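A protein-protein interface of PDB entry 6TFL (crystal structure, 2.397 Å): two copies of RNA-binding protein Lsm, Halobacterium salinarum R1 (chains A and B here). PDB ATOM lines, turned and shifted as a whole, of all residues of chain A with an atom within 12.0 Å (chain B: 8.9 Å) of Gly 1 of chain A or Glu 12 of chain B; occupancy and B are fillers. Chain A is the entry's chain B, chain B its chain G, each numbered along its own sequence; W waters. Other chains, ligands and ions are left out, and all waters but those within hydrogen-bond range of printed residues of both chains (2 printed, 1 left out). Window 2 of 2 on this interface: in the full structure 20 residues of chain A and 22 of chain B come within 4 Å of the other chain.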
ATOM      1  N   GLY A   1      31.218  38.848   8.594  1.00  0.00           N
ATOM      2  CA  GLY A   1      32.174  37.989   9.271  1.00  0.00           C
ATOM      3  C   GLY A   1      32.158  36.540   8.810  1.00  0.00           C
ATOM      4  O   GLY A   1      31.700  36.233   7.709  1.00  0.00           O
ATOM      5  N   ALA A   2      32.670  35.640   9.645  1.00  0.00           N
ATOM      6  CA  ALA A   2      32.626  34.219   9.340  1.00  0.00           C
ATOM      7  C   ALA A   2      31.398  33.586   9.978  1.00  0.00           C
ATOM      8  O   ALA A   2      30.753  34.168  10.852  1.00  0.00           O
ATOM      9  CB  ALA A   2      33.897  33.513   9.817  1.00  0.00           C
ATOM     10  N   MET A   3      31.063  32.391   9.495  1.00  0.00           N
ATOM     11  CA  MET A   3      30.060  31.503  10.071  1.00  0.00           C
ATOM     12  C   MET A   3      28.629  31.970   9.842  1.00  0.00           C
ATOM     13  O   MET A   3      27.696  31.343  10.363  1.00  0.00           O
ATOM     14  CB  MET A   3      30.318  31.282  11.572  1.00  0.00           C
ATOM     15  CG  MET A   3      31.597  30.472  11.800  1.00  0.00           C
ATOM     16  SD  MET A   3      32.097  30.175  13.496  1.00  0.00           S
ATOM     17  CE  MET A   3      33.114  28.710  13.291  1.00  0.00           C
ATOM     18  N   SER A   4      28.419  33.033   9.069  1.00  0.00           N
ATOM     19  CA  SER A   4      27.061  33.456   8.765  1.00  0.00           C
ATOM     20  C   SER A   4      26.322  33.921  10.006  1.00  0.00           C
ATOM     21  O   SER A   4      26.870  34.609  10.875  1.00  0.00           O
ATOM     22  N   GLY A   5      25.047  33.572  10.080  1.00  0.00           N
ATOM     23  CA  GLY A   5      24.314  33.775  11.316  1.00  0.00           C
ATOM     24  C   GLY A   5      24.490  32.567  12.210  1.00  0.00           C
ATOM     25  O   GLY A   5      23.804  31.566  12.006  1.00  0.00           O
ATOM     26  N   ARG A   6      25.436  32.614  13.154  1.00  0.00           N
ATOM     27  CA  ARG A   6      25.743  31.471  14.023  1.00  0.00           C
ATOM     28  C   ARG A   6      24.487  30.920  14.689  1.00  0.00           C
ATOM     29  O   ARG A   6      23.563  31.688  14.995  1.00  0.00           O
ATOM     30  CB  ARG A   6      26.749  31.857  15.110  1.00  0.00           C
ATOM     31  CG  ARG A   6      28.125  32.164  14.608  1.00  0.00           C
ATOM     32  CD  ARG A   6      28.916  32.962  15.630  1.00  0.00           C
ATOM     33  NE  ARG A   6      30.291  33.202  15.177  1.00  0.00           N
ATOM     34  CZ  ARG A   6      30.672  34.236  14.433  1.00  0.00           C
ATOM     35  NH1 ARG A   6      29.788  35.156  14.035  1.00  0.00           N
ATOM     36  NH2 ARG A   6      31.946  34.355  14.086  1.00  0.00           N
ATOM     37  N   PRO A   7      24.419  29.601  14.912  1.00  0.00           N
ATOM     38  CA  PRO A   7      23.258  29.006  15.627  1.00  0.00           C
ATOM     39  C   PRO A   7      22.918  29.645  16.975  1.00  0.00           C
ATOM     40  O   PRO A   7      21.730  29.813  17.293  1.00  0.00           O
ATOM     41  CB  PRO A   7      23.680  27.541  15.803  1.00  0.00           C
ATOM     42  CG  PRO A   7      24.626  27.277  14.637  1.00  0.00           C
ATOM     43  CD  PRO A   7      25.363  28.585  14.410  1.00  0.00           C
ATOM     44  N   ASP A   9      23.539  32.724  17.789  1.00  0.00           N
ATOM     45  CA  ASP A   9      23.029  34.053  17.483  1.00  0.00           C
ATOM     46  C   ASP A   9      21.576  33.994  17.036  1.00  0.00           C
ATOM     47  O   ASP A   9      20.764  34.835  17.433  1.00  0.00           O
ATOM     48  CB  ASP A   9      23.899  34.719  16.418  1.00  0.00           C
ATOM     49  CG  ASP A   9      25.123  35.395  17.017  1.00  0.00           C
ATOM     50  OD1 ASP A   9      25.182  35.495  18.265  1.00  0.00           O
ATOM     51  OD2 ASP A   9      26.025  35.819  16.259  1.00  0.00           O
ATOM     52  N   ARG B   6      39.673  22.364   4.876  1.00  0.00           N
ATOM     53  CA  ARG B   6      39.113  21.980   6.172  1.00  0.00           C
ATOM     54  C   ARG B   6      37.593  21.803   6.086  1.00  0.00           C
ATOM     55  O   ARG B   6      36.924  22.536   5.348  1.00  0.00           O
ATOM     56  CB  ARG B   6      39.441  23.035   7.238  1.00  0.00           C
ATOM     57  CG  ARG B   6      40.879  23.015   7.758  1.00  0.00           C
ATOM     58  CD  ARG B   6      41.205  24.362   8.435  1.00  0.00           C
ATOM     59  NE  ARG B   6      42.550  24.400   8.997  1.00  0.00           N
ATOM     60  CZ  ARG B   6      43.636  24.749   8.314  1.00  0.00           C
ATOM     61  NH1 ARG B   6      43.537  25.109   7.036  1.00  0.00           N
ATOM     62  NH2 ARG B   6      44.821  24.739   8.907  1.00  0.00           N
ATOM     63  N   PRO B   7      37.022  20.834   6.813  1.00  0.00           N
ATOM     64  CA  PRO B   7      35.554  20.669   6.811  1.00  0.00           C
ATOM     65  C   PRO B   7      34.789  21.939   7.142  1.00  0.00           C
ATOM     66  O   PRO B   7      33.778  22.235   6.493  1.00  0.00           O
ATOM     67  CB  PRO B   7      35.333  19.577   7.872  1.00  0.00           C
ATOM     68  CG  PRO B   7      36.610  18.766   7.815  1.00  0.00           C
ATOM     69  CD  PRO B   7      37.701  19.775   7.584  1.00  0.00           C
ATOM     70  N   LEU B   8      35.235  22.699   8.143  1.00  0.00           N
ATOM     71  CA  LEU B   8      34.537  23.935   8.465  1.00  0.00           C
ATOM     72  C   LEU B   8      34.706  24.972   7.361  1.00  0.00           C
ATOM     73  O   LEU B   8      33.799  25.782   7.132  1.00  0.00           O
ATOM     74  CB  LEU B   8      35.020  24.489   9.809  1.00  0.00           C
ATOM     75  CG  LEU B   8      34.685  23.664  11.055  1.00  0.00           C
ATOM     76  CD1 LEU B   8      34.706  24.525  12.308  1.00  0.00           C
ATOM     77  CD2 LEU B   8      33.341  22.985  10.908  1.00  0.00           C
ATOM     78  N   ASP B   9      35.846  24.964   6.670  1.00  0.00           N
ATOM     79  CA  ASP B   9      36.028  25.867   5.539  1.00  0.00           C
ATOM     80  C   ASP B   9      35.117  25.498   4.372  1.00  0.00           C
ATOM     81  O   ASP B   9      34.618  26.388   3.674  1.00  0.00           O
ATOM     82  CB  ASP B   9      37.492  25.885   5.108  1.00  0.00           C
ATOM     83  CG  ASP B   9      38.327  26.841   5.949  1.00  0.00           C
ATOM     84  OD1 ASP B   9      37.749  27.503   6.842  1.00  0.00           O
ATOM     85  OD2 ASP B   9      39.553  26.934   5.729  1.00  0.00           O
ATOM     86  N   VAL B  10      34.873  24.203   4.146  1.00  0.00           N
ATOM     87  CA  VAL B  10      33.852  23.824   3.167  1.00  0.00           C
ATOM     88  C   VAL B  10      32.491  24.381   3.585  1.00  0.00           C
ATOM     89  O   VAL B  10      31.711  24.849   2.746  1.00  0.00           O
ATOM     90  CB  VAL B  10      33.810  22.291   2.978  1.00  0.00           C
ATOM     91  CG1 VAL B  10      32.657  21.884   2.050  1.00  0.00           C
ATOM     92  CG2 VAL B  10      35.154  21.750   2.450  1.00  0.00           C
ATOM     93  N   LEU B  11      32.190  24.361   4.888  1.00  0.00           N
ATOM     94  CA  LEU B  11      30.940  24.951   5.366  1.00  0.00           C
ATOM     95  C   LEU B  11      30.894  26.448   5.080  1.00  0.00           C
ATOM     96  O   LEU B  11      29.886  26.958   4.577  1.00  0.00           O
ATOM     97  CB  LEU B  11      30.755  24.684   6.862  1.00  0.00           C
ATOM     98  CG  LEU B  11      30.251  23.288   7.230  1.00  0.00           C
ATOM     99  CD1 LEU B  11      29.715  23.222   8.679  1.00  0.00           C
ATOM    100  CD2 LEU B  11      29.195  22.834   6.230  1.00  0.00           C
ATOM    101  N   GLU B  12      31.970  27.177   5.412  1.00  0.00           N
ATOM    102  CA  GLU B  12      32.014  28.611   5.119  1.00  0.00           C
ATOM    103  C   GLU B  12      31.695  28.886   3.657  1.00  0.00           C
ATOM    104  O   GLU B  12      30.858  29.736   3.343  1.00  0.00           O
ATOM    105  CB  GLU B  12      33.380  29.199   5.470  1.00  0.00           C
ATOM    106  CG  GLU B  12      33.439  30.702   5.270  1.00  0.00           C
ATOM    107  CD  GLU B  12      32.729  31.473   6.391  1.00  0.00           C
ATOM    108  OE1 GLU B  12      32.492  30.873   7.472  1.00  0.00           O
ATOM    109  OE2 GLU B  12      32.404  32.671   6.190  1.00  0.00           O
ATOM    110  N   GLU B  13      32.328  28.133   2.749  1.00  0.00           N
ATOM    111  CA  GLU B  13      32.102  28.264   1.314  1.00  0.00           C
ATOM    112  C   GLU B  13      30.697  27.851   0.886  1.00  0.00           C
ATOM    113  O   GLU B  13      30.301  28.143  -0.244  1.00  0.00           O
ATOM    114  CB  GLU B  13      33.137  27.431   0.558  1.00  0.00           C
ATOM    115  CG  GLU B  13      34.583  27.965   0.614  1.00  0.00           C
ATOM    116  CD  GLU B  13      35.638  26.870   0.350  1.00  0.00           C
ATOM    117  OE1 GLU B  13      36.814  27.035   0.763  1.00  0.00           O
ATOM    118  OE2 GLU B  13      35.284  25.836  -0.265  1.00  0.00           O
ATOM    119  N   SER B  14      29.936  27.185   1.748  1.00  0.00           N
ATOM    120  CA  SER B  14      28.567  26.786   1.449  1.00  0.00           C
ATOM    121  C   SER B  14      27.499  27.731   2.008  1.00  0.00           C
ATOM    122  O   SER B  14      26.309  27.462   1.818  1.00  0.00           O
ATOM    123  CB  SER B  14      28.317  25.384   1.989  1.00  0.00           C
ATOM    124  OG  SER B  14      29.225  24.459   1.420  1.00  0.00           O
ATOM    125  N   LEU B  15      27.878  28.816   2.689  1.00  0.00           N
ATOM    126  CA  LEU B  15      26.881  29.763   3.192  1.00  0.00           C
ATOM    127  C   LEU B  15      26.085  30.374   2.048  1.00  0.00           C
ATOM    128  O   LEU B  15      26.637  30.733   1.006  1.00  0.00           O
ATOM    129  CB  LEU B  15      27.541  30.874   4.013  1.00  0.00           C
ATOM    130  CG  LEU B  15      28.187  30.402   5.313  1.00  0.00           C
ATOM    131  CD1 LEU B  15      29.081  31.490   5.876  1.00  0.00           C
ATOM    132  CD2 LEU B  15      27.144  29.957   6.315  1.00  0.00           C
ATOM    133  N   GLU B  16      24.778  30.504   2.260  1.00  0.00           N
ATOM    134  CA  GLU B  16      23.835  31.004   1.259  1.00  0.00           C
ATOM    135  C   GLU B  16      23.727  30.078   0.066  1.00  0.00           C
ATOM    136  O   GLU B  16      23.273  30.488  -1.002  1.00  0.00           O
ATOM    137  CB  GLU B  16      24.180  32.424   0.781  1.00  0.00           C
ATOM    138  CG  GLU B  16      23.858  33.495   1.803  1.00  0.00           C
ATOM    139  CD  GLU B  16      25.067  33.861   2.628  1.00  0.00           C
ATOM    140  OE1 GLU B  16      26.101  34.226   2.025  1.00  0.00           O
ATOM    141  OE2 GLU B  16      24.990  33.760   3.876  1.00  0.00           O
ATOM    142  N   GLU B  17      24.125  28.827   0.238  1.00  0.00           N
ATOM    143  CA  GLU B  17      23.927  27.805  -0.770  1.00  0.00           C
ATOM    144  C   GLU B  17      23.141  26.666  -0.147  1.00  0.00           C
ATOM    145  O   GLU B  17      23.163  26.467   1.075  1.00  0.00           O
ATOM    146  CB  GLU B  17      25.267  27.322  -1.334  1.00  0.00           C
ATOM    147  CG  GLU B  17      26.007  28.423  -2.087  1.00  0.00           C
ATOM    148  CD  GLU B  17      27.417  28.028  -2.504  1.00  0.00           C
ATOM    149  OE1 GLU B  17      27.789  26.864  -2.276  1.00  0.00           O
ATOM    150  OE2 GLU B  17      28.148  28.880  -3.065  1.00  0.00           O
ATOM    151  N   VAL B  19      22.338  22.970   0.940  1.00  0.00           N
ATOM    152  CA  VAL B  19      23.066  21.770   1.350  1.00  0.00           C
ATOM    153  C   VAL B  19      22.059  20.754   1.867  1.00  0.00           C
ATOM    154  O   VAL B  19      20.862  21.037   1.978  1.00  0.00           O
ATOM    155  CB  VAL B  19      24.129  22.061   2.431  1.00  0.00           C
ATOM    156  CG1 VAL B  19      25.068  23.170   1.984  1.00  0.00           C
ATOM    157  CG2 VAL B  19      23.453  22.407   3.762  1.00  0.00           C
ATOM    158  N   LEU B  33      22.174  26.784   3.743  1.00  0.00           N
ATOM    159  CA  LEU B  33      23.048  26.902   4.902  1.00  0.00           C
ATOM    160  C   LEU B  33      23.210  28.389   5.199  1.00  0.00           C
ATOM    161  O   LEU B  33      23.841  29.106   4.420  1.00  0.00           O
ATOM    162  CB  LEU B  33      24.393  26.221   4.639  1.00  0.00           C
ATOM    163  CG  LEU B  33      25.379  26.265   5.818  1.00  0.00           C
ATOM    164  CD1 LEU B  33      24.888  25.417   7.015  1.00  0.00           C
ATOM    165  CD2 LEU B  33      26.784  25.861   5.404  1.00  0.00           C
ATOM    166  N   THR B  34      22.625  28.857   6.313  1.00  0.00           N
ATOM    167  CA  THR B  34      22.723  30.264   6.704  1.00  0.00           C
ATOM    168  C   THR B  34      23.671  30.506   7.875  1.00  0.00           C
ATOM    169  O   THR B  34      24.051  31.659   8.117  1.00  0.00           O
ATOM    170  CB  THR B  34      21.342  30.840   7.076  1.00  0.00           C
ATOM    171  OG1 THR B  34      20.787  30.094   8.160  1.00  0.00           O
ATOM    172  CG2 THR B  34      20.361  30.801   5.901  1.00  0.00           C
ATOM    173  N   GLY B  35      24.052  29.467   8.612  1.00  0.00           N
ATOM    174  CA  GLY B  35      25.013  29.636   9.685  1.00  0.00           C
ATOM    175  C   GLY B  35      25.545  28.302  10.154  1.00  0.00           C
ATOM    176  O   GLY B  35      24.958  27.246   9.894  1.00  0.00           O
ATOM    177  N   TYR B  36      26.662  28.365  10.863  1.00  0.00           N
ATOM    178  CA  TYR B  36      27.252  27.179  11.466  1.00  0.00           C
ATOM    179  C   TYR B  36      28.203  27.656  12.547  1.00  0.00           C
ATOM    180  O   TYR B  36      28.562  28.837  12.595  1.00  0.00           O
ATOM    181  CB  TYR B  36      27.982  26.294  10.429  1.00  0.00           C
ATOM    182  CG  TYR B  36      29.273  26.898   9.966  1.00  0.00           C
ATOM    183  CD1 TYR B  36      30.474  26.653  10.644  1.00  0.00           C
ATOM    184  CD2 TYR B  36      29.300  27.735   8.848  1.00  0.00           C
ATOM    185  CE1 TYR B  36      31.659  27.236  10.219  1.00  0.00           C
ATOM    186  CE2 TYR B  36      30.486  28.321   8.413  1.00  0.00           C
ATOM    187  CZ  TYR B  36      31.652  28.069   9.098  1.00  0.00           C
ATOM    188  OH  TYR B  36      32.802  28.659   8.658  1.00  0.00           O
ATOM    189  N   ASP B  37      28.620  26.726  13.419  1.00  0.00           N
ATOM    190  CA  ASP B  37      29.662  27.058  14.382  1.00  0.00           C
ATOM    191  C   ASP B  37      30.692  25.935  14.452  1.00  0.00           C
ATOM    192  O   ASP B  37      30.633  24.960  13.709  1.00  0.00           O
ATOM    193  CB  ASP B  37      29.071  27.396  15.754  1.00  0.00           C
ATOM    194  CG  ASP B  37      28.257  26.254  16.366  1.00  0.00           C
ATOM    195  OD1 ASP B  37      28.481  25.054  16.048  1.00  0.00           O
ATOM    196  OD2 ASP B  37      27.366  26.590  17.184  1.00  0.00           O
HETATM  197  O   HOH W   1      21.777  31.483  10.287  1.00  0.00           O
HETATM  198  O   HOH W   2      30.186  34.267   6.879  1.00  0.00           O
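The backbone NH (N) of Met 3 of chain A is in hydrogen-bond range of the side-chain carboxylate (OE1) of Glu 12 of chain B (2.9 Å).
The backbone NH (N) of Tyr 36 of chain B sits at hydrogen-bond distance from the backbone carbonyl oxygen (O) of Met 3 of chain A.
The backbone carbonyl oxygen (O) of Thr 34 of chain B is in hydrogen-bond range of the backbone NH (N) of Gly 5 of chain A, 2.9 Å away.
The backbone carbonyl oxygen (O) of Ala 2 of chain A lies within hydrogen-bond range of the guanidinium group (NH2) of Arg 6 of chain A, 3.5 Å away.
OH of Tyr 36 of chain B lies within hydrogen-bond range of O of Leu 8 of chain B.
The side-chain hydroxyl of Tyr 36 of chain B is in hydrogen-bond range of the side-chain carboxylate of Glu 12 of chain B, 2.5 Å away.
Gly 1 of chain A touches Glu 12 of chain B (O to OE2, 3.9 Å).
Ala 2 of chain A touches Glu 12 of chain B.
Gly 35 of chain B touches Met 3 of chain A.
C of Asp 37 of chain B touches CE of Met 3 of chain A (3.9 Å).
CD1 of Leu 15 of chain B touches N of Ser 4 of chain A, 3.6 Å away.
Thr 34 of chain B touches Ser 4 of chain A.
Gly 5 of chain A touches Gly 35 of chain B (O to CA, 3.3 Å).
Tyr 36 of chain B touches Arg 6 of chain A (O to CG, 3.9 Å).
Tyr 36 of chain B touches Pro 7 of chain A.
CG of Pro 7 of chain A touches OD2 of Asp 37 of chain B (3.8 Å).
Printed residues of chain B within 4 Å of Arg 6 of chain A: Tyr 36 (3.9 Å).
Leu 8 of chain B touches none of the printed residues of chain A.
No residue of chain A comes within 4 Å of Asp 9 of chain B.
Leu 11 of chain B touches none of the printed residues of chain A.
Glu 12 of chain B touches just these residues of chain A: Gly 1, Ala 2 and Met 3.
No residue of chain A comes within 4 Å of Glu 13 of chain B.
Printed residues of chain A within 4 Å of Leu 15 of chain B: Ser 4.
Of the printed residues of chain A, Thr 34 of chain B touches Ser 4 and Gly 5.
Of the printed residues of chain A, Gly 35 of chain B touches Met 3 (3.3 Å) and Gly 5 (3.3 Å).
Printed residues of chain A within 4 Å of Asp 37 of chain B: Met 3 and Pro 7.
Of the 8 printed residues of chain A, 7 touch a printed residue of chain B.
Hydrophobic or aromatic side chains of chain A that line the printed part of chain B: Ala 2, Met 3 and Pro 7.
Among the printed residues, no Asp or Glu carboxylate lies within 4 Å of a Lys or Arg side-chain nitrogen of the other chain.
Positions printed for both chains: 6, 7 and 9.
Of the 13 pairs that touch across the chains among the printed residues, none has its exchanged pair printed and touching as well.
Water W2 lies within hydrogen-bond range of O of Gly 1 of chain A, OE2 of Glu 12 of chain B, N of Ser 4 of chain A and N of Met 3 of chain A.
Water W1 lies within hydrogen-bond range of the backbone carbonyl oxygen (O) of Gly 5 of chain A (2.7 Å), the side-chain hydroxyl (OG1) of Thr 34 of chain B (2.7 Å) and the backbone NH (N) of Gly 35 of chain B (3.5 Å).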
